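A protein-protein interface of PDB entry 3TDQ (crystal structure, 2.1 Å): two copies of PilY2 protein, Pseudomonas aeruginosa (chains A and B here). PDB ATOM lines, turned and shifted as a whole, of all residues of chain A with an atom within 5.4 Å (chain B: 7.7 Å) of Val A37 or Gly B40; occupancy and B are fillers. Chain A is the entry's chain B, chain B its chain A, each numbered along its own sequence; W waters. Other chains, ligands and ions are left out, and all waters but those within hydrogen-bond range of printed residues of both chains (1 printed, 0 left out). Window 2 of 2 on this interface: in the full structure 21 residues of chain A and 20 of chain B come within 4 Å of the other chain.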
ATOM      1  N   ASN A  34       4.685  12.329 -29.570  1.00  0.00           N
ATOM      2  CA  ASN A  34       3.886  13.300 -28.840  1.00  0.00           C
ATOM      3  C   ASN A  34       2.393  13.130 -29.117  1.00  0.00           C
ATOM      4  O   ASN A  34       1.603  13.616 -28.330  1.00  0.00           O
ATOM      5  CB  ASN A  34       4.308  14.743 -29.173  1.00  0.00           C
ATOM      6  CG  ASN A  34       5.592  15.178 -28.509  1.00  0.00           C
ATOM      7  OD1 ASN A  34       6.467  14.397 -28.165  1.00  0.00           O
ATOM      8  ND2 ASN A  34       5.731  16.465 -28.319  1.00  0.00           N
ATOM      9  N   SER A  35       1.999  12.459 -30.211  1.00  0.00           N
ATOM     10  CA  SER A  35       0.599  12.204 -30.569  1.00  0.00           C
ATOM     11  C   SER A  35      -0.059  11.164 -29.635  1.00  0.00           C
ATOM     12  O   SER A  35      -1.282  11.048 -29.635  1.00  0.00           O
ATOM     13  CB  SER A  35       0.483  11.775 -32.030  1.00  0.00           C
ATOM     14  OG  SER A  35       1.240  10.596 -32.266  1.00  0.00           O
ATOM     15  N   THR A  36       0.721  10.436 -28.811  1.00  0.00           N
ATOM     16  CA  THR A  36       0.151   9.511 -27.808  1.00  0.00           C
ATOM     17  C   THR A  36      -0.168  10.427 -26.602  1.00  0.00           C
ATOM     18  O   THR A  36       0.749  10.822 -25.856  1.00  0.00           O
ATOM     19  CB  THR A  36       1.123   8.379 -27.556  1.00  0.00           C
ATOM     20  OG1 THR A  36       1.386   7.726 -28.803  1.00  0.00           O
ATOM     21  CG2 THR A  36       0.572   7.412 -26.570  1.00  0.00           C
ATOM     22  N   VAL A  37      -1.462  10.818 -26.477  1.00  0.00           N
ATOM     23  CA  VAL A  37      -1.924  11.839 -25.531  1.00  0.00           C
ATOM     24  C   VAL A  37      -3.106  11.360 -24.659  1.00  0.00           C
ATOM     25  O   VAL A  37      -3.991  10.629 -25.120  1.00  0.00           O
ATOM     26  CB  VAL A  37      -2.293  13.138 -26.349  1.00  0.00           C
ATOM     27  CG1 VAL A  37      -3.615  13.039 -27.090  1.00  0.00           C
ATOM     28  CG2 VAL A  37      -2.230  14.409 -25.512  1.00  0.00           C
ATOM     29  N   ARG A  38      -3.146  11.864 -23.432  1.00  0.00           N
ATOM     30  CA  ARG A  38      -4.198  11.618 -22.461  1.00  0.00           C
ATOM     31  C   ARG A  38      -4.473  12.948 -21.784  1.00  0.00           C
ATOM     32  O   ARG A  38      -3.523  13.630 -21.387  1.00  0.00           O
ATOM     33  CB  ARG A  38      -3.757  10.525 -21.474  1.00  0.00           C
ATOM     34  CG  ARG A  38      -4.672  10.367 -20.281  1.00  0.00           C
ATOM     35  CD  ARG A  38      -3.928   9.827 -19.086  1.00  0.00           C
ATOM     36  NE  ARG A  38      -3.478  10.883 -18.180  1.00  0.00           N
ATOM     37  CZ  ARG A  38      -4.190  11.344 -17.159  1.00  0.00           C
ATOM     38  NH1 ARG A  38      -5.404  10.868 -16.919  1.00  0.00           N
ATOM     39  NH2 ARG A  38      -3.699  12.293 -16.376  1.00  0.00           N
ATOM     40  N   ASN A  39      -5.764  13.352 -21.719  1.00  0.00           N
ATOM     41  CA  ASN A  39      -6.241  14.601 -21.118  1.00  0.00           C
ATOM     42  C   ASN A  39      -5.389  15.813 -21.559  1.00  0.00           C
ATOM     43  O   ASN A  39      -4.988  16.649 -20.738  1.00  0.00           O
ATOM     44  CB  ASN A  39      -6.330  14.478 -19.588  1.00  0.00           C
ATOM     45  CG  ASN A  39      -7.386  13.499 -19.122  1.00  0.00           C
ATOM     46  OD1 ASN A  39      -8.267  13.058 -19.872  1.00  0.00           O
ATOM     47  ND2 ASN A  39      -7.319  13.127 -17.861  1.00  0.00           N
ATOM     48  N   GLY A  40      -5.130  15.879 -22.865  1.00  0.00           N
ATOM     49  CA  GLY A  40      -4.368  16.956 -23.487  1.00  0.00           C
ATOM     50  C   GLY A  40      -2.876  16.964 -23.225  1.00  0.00           C
ATOM     51  O   GLY A  40      -2.194  17.869 -23.704  1.00  0.00           O
ATOM     52  N   MET A  41      -2.342  15.954 -22.511  1.00  0.00           N
ATOM     53  CA  MET A  41      -0.916  15.882 -22.179  1.00  0.00           C
ATOM     54  C   MET A  41      -0.200  14.678 -22.812  1.00  0.00           C
ATOM     55  O   MET A  41      -0.623  13.534 -22.581  1.00  0.00           O
ATOM     56  CB  MET A  41      -0.726  15.814 -20.659  1.00  0.00           C
ATOM     57  CG  MET A  41      -1.303  17.018 -19.907  1.00  0.00           C
ATOM     58  SD  MET A  41      -1.426  16.683 -17.962  1.00  0.00           S
ATOM     59  CE  MET A  41      -2.592  15.134 -17.948  1.00  0.00           C
ATOM     60  N   PRO A  42       0.909  14.904 -23.573  1.00  0.00           N
ATOM     61  CA  PRO A  42       1.640  13.765 -24.155  1.00  0.00           C
ATOM     62  C   PRO A  42       2.141  12.812 -23.079  1.00  0.00           C
ATOM     63  O   PRO A  42       2.763  13.243 -22.106  1.00  0.00           O
ATOM     64  CB  PRO A  42       2.786  14.425 -24.917  1.00  0.00           C
ATOM     65  CG  PRO A  42       2.321  15.835 -25.173  1.00  0.00           C
ATOM     66  CD  PRO A  42       1.541  16.188 -23.945  1.00  0.00           C
ATOM     67  N   SER A  43       1.838  11.520 -23.242  1.00  0.00           N
ATOM     68  CA  SER A  43       2.233  10.471 -22.286  1.00  0.00           C
ATOM     69  C   SER A  43       3.746  10.387 -22.110  1.00  0.00           C
ATOM     70  O   SER A  43       4.199   9.960 -21.053  1.00  0.00           O
ATOM     71  CB  SER A  43       1.697   9.119 -22.735  1.00  0.00           C
ATOM     72  OG  SER A  43       0.288   9.177 -22.869  1.00  0.00           O
ATOM     73  N   ASN B  34     -17.028  13.954 -20.370  1.00  0.00           N
ATOM     74  CA  ASN B  34     -16.448  14.213 -21.708  1.00  0.00           C
ATOM     75  C   ASN B  34     -14.990  14.682 -21.616  1.00  0.00           C
ATOM     76  O   ASN B  34     -14.257  14.535 -22.572  1.00  0.00           O
ATOM     77  CB  ASN B  34     -17.287  15.291 -22.438  1.00  0.00           C
ATOM     78  CG  ASN B  34     -18.721  14.894 -22.753  1.00  0.00           C
ATOM     79  OD1 ASN B  34     -19.122  13.706 -22.651  1.00  0.00           O
ATOM     80  ND2 ASN B  34     -19.535  15.901 -23.094  1.00  0.00           N
ATOM     81  N   THR B  36     -12.645  13.295 -19.905  1.00  0.00           N
ATOM     82  CA  THR B  36     -11.725  12.135 -19.867  1.00  0.00           C
ATOM     83  C   THR B  36     -11.508  11.806 -21.320  1.00  0.00           C
ATOM     84  O   THR B  36     -12.379  11.199 -21.974  1.00  0.00           O
ATOM     85  CB  THR B  36     -12.298  11.005 -19.017  1.00  0.00           C
ATOM     86  OG1 THR B  36     -12.510  11.559 -17.716  1.00  0.00           O
ATOM     87  CG2 THR B  36     -11.370   9.762 -18.965  1.00  0.00           C
ATOM     88  N   VAL B  37     -10.366  12.256 -21.847  1.00  0.00           N
ATOM     89  CA  VAL B  37     -10.018  12.194 -23.258  1.00  0.00           C
ATOM     90  C   VAL B  37      -8.674  11.466 -23.471  1.00  0.00           C
ATOM     91  O   VAL B  37      -7.731  11.647 -22.704  1.00  0.00           O
ATOM     92  CB  VAL B  37      -9.995  13.652 -23.824  1.00  0.00           C
ATOM     93  CG1 VAL B  37      -9.605  13.699 -25.293  1.00  0.00           C
ATOM     94  CG2 VAL B  37     -11.315  14.379 -23.607  1.00  0.00           C
ATOM     95  N   ARG B  38      -8.610  10.646 -24.529  1.00  0.00           N
ATOM     96  CA  ARG B  38      -7.434   9.892 -24.930  1.00  0.00           C
ATOM     97  C   ARG B  38      -7.322  10.047 -26.453  1.00  0.00           C
ATOM     98  O   ARG B  38      -8.299   9.814 -27.175  1.00  0.00           O
ATOM     99  CB  ARG B  38      -7.571   8.417 -24.478  1.00  0.00           C
ATOM    100  CG  ARG B  38      -6.266   7.637 -24.326  1.00  0.00           C
ATOM    101  CD  ARG B  38      -6.493   6.287 -23.597  1.00  0.00           C
ATOM    102  NE  ARG B  38      -5.391   5.962 -22.681  1.00  0.00           N
ATOM    103  CZ  ARG B  38      -5.373   6.288 -21.401  1.00  0.00           C
ATOM    104  NH1 ARG B  38      -6.435   6.853 -20.838  1.00  0.00           N
ATOM    105  NH2 ARG B  38      -4.308   6.034 -20.663  1.00  0.00           N
ATOM    106  N   ASN B  39      -6.173  10.545 -26.924  1.00  0.00           N
ATOM    107  CA  ASN B  39      -5.878  10.796 -28.346  1.00  0.00           C
ATOM    108  C   ASN B  39      -6.937  11.712 -28.997  1.00  0.00           C
ATOM    109  O   ASN B  39      -7.403  11.433 -30.101  1.00  0.00           O
ATOM    110  CB  ASN B  39      -5.674   9.479 -29.124  1.00  0.00           C
ATOM    111  CG  ASN B  39      -4.482   8.682 -28.619  1.00  0.00           C
ATOM    112  OD1 ASN B  39      -3.546   9.224 -28.015  1.00  0.00           O
ATOM    113  ND2 ASN B  39      -4.518   7.363 -28.789  1.00  0.00           N
ATOM    114  N   GLY B  40      -7.288  12.791 -28.288  1.00  0.00           N
ATOM    115  CA  GLY B  40      -8.269  13.784 -28.724  1.00  0.00           C
ATOM    116  C   GLY B  40      -9.731  13.349 -28.750  1.00  0.00           C
ATOM    117  O   GLY B  40     -10.593  14.135 -29.139  1.00  0.00           O
ATOM    118  N   MET B  41     -10.040  12.117 -28.314  1.00  0.00           N
ATOM    119  CA  MET B  41     -11.409  11.584 -28.340  1.00  0.00           C
ATOM    120  C   MET B  41     -11.931  11.242 -26.929  1.00  0.00           C
ATOM    121  O   MET B  41     -11.245  10.520 -26.202  1.00  0.00           O
ATOM    122  CB  MET B  41     -11.462  10.315 -29.210  1.00  0.00           C
ATOM    123  CG  MET B  41     -11.054  10.542 -30.658  1.00  0.00           C
ATOM    124  SD  MET B  41     -10.802   8.861 -31.574  1.00  0.00           S
ATOM    125  CE  MET B  41      -9.279   8.121 -30.546  1.00  0.00           C
ATOM    126  N   PRO B  42     -13.164  11.665 -26.547  1.00  0.00           N
ATOM    127  CA  PRO B  42     -13.684  11.295 -25.215  1.00  0.00           C
ATOM    128  C   PRO B  42     -13.776   9.778 -25.065  1.00  0.00           C
ATOM    129  O   PRO B  42     -14.315   9.080 -25.937  1.00  0.00           O
ATOM    130  CB  PRO B  42     -15.067  11.977 -25.151  1.00  0.00           C
ATOM    131  CG  PRO B  42     -14.992  13.056 -26.159  1.00  0.00           C
ATOM    132  CD  PRO B  42     -14.118  12.523 -27.270  1.00  0.00           C
ATOM    133  N   SER B  43     -13.196   9.249 -23.978  1.00  0.00           N
ATOM    134  CA  SER B  43     -13.197   7.795 -23.707  1.00  0.00           C
ATOM    135  C   SER B  43     -14.620   7.225 -23.587  1.00  0.00           C
ATOM    136  O   SER B  43     -14.827   6.037 -23.818  1.00  0.00           O
ATOM    137  CB  SER B  43     -12.412   7.483 -22.437  1.00  0.00           C
ATOM    138  OG  SER B  43     -11.078   7.958 -22.540  1.00  0.00           O
HETATM  139  O   HOH W   1      -7.798  10.259 -20.103  1.00  0.00           O
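The backbone carbonyl oxygen of Val B37 lies within hydrogen-bond range of the backbone NH of Asn A39 (2.8 Å).
The backbone NH (N) of Asn B39 lies within hydrogen-bond range of the backbone carbonyl oxygen (O) of Val A37 (2.8 Å).
OD1 of Asn B39 lies close to O of Ser A35, 3.3 Å away.
N of Ser A43 sits at hydrogen-bond distance from O of Thr A36 (2.9 Å).
O of Thr B36 lies within hydrogen-bond range of N of Ser B43 (2.9 Å).
The guanidinium group of Arg A38 lies close to the side-chain amide nitrogen of Asn A39, at 3.1 Å.
Thr A36 touches Asn B39 (CA to OD1, 3.7 Å).
O of Val A37 touches CA of Arg B38, 3.5 Å away.
N of Gly B40 touches CG1 of Val A37, 3.9 Å away.
O of Val B37 touches CA of Arg A38, at 3.5 Å.
NH1 of Arg B38 touches CG of Arg A38 (3.97 Å).
OD1 of Asn A39 touches CA of Thr B36, 3.6 Å away.
Printed residues of chain B within 4 Å of Val A37: Arg B38, Asn B39 and Gly B40.
Of the printed residues of chain A, Gly B40 touches Val A37 (3.9 Å).
Of the printed residues of chain A, Arg B38 touches Val A37 (3.5 Å) and Arg A38 (3.97 Å).
Of the printed residues of chain B, Ser A35 touches Asn B39 (3.3 Å).
Printed residues of chain A within 4 Å of Asn B39: Ser A35 (3.3 Å), Thr A36 (3.7 Å) and Val A37 (2.8 Å).
Printed residues of chain B within 4 Å of Asn A39: Thr B36 and Val B37.
Met B41 touches none of the printed residues of chain A.
The nearest printed residue of chain B that does not touch Thr A36 is Arg B38 (7.1 Å).
Hydrophobic or aromatic side chains of chain A within 4 Å of the printed part of chain B: Val A37.
Thr A36 touches Asn B39, and with the chains exchanged Asn A39 touches Thr B36.
Val A37 touches Asn B39, and with the chains exchanged Asn A39 touches Val B37.
Val A37 touches Gly B40, but with the chains exchanged Gly A40 does not touch Val B37 (5.0 Å).
Arg A38 touches its own counterpart, Arg B38.
Of the 9 pairs that touch across the chains among the printed residues, 7 have their exchanged pair printed and touching as well.
Water W1 lies within hydrogen-bond range of OD1 of Asn A39 (2.8 Å) and O of Val B37 (2.9 Å).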
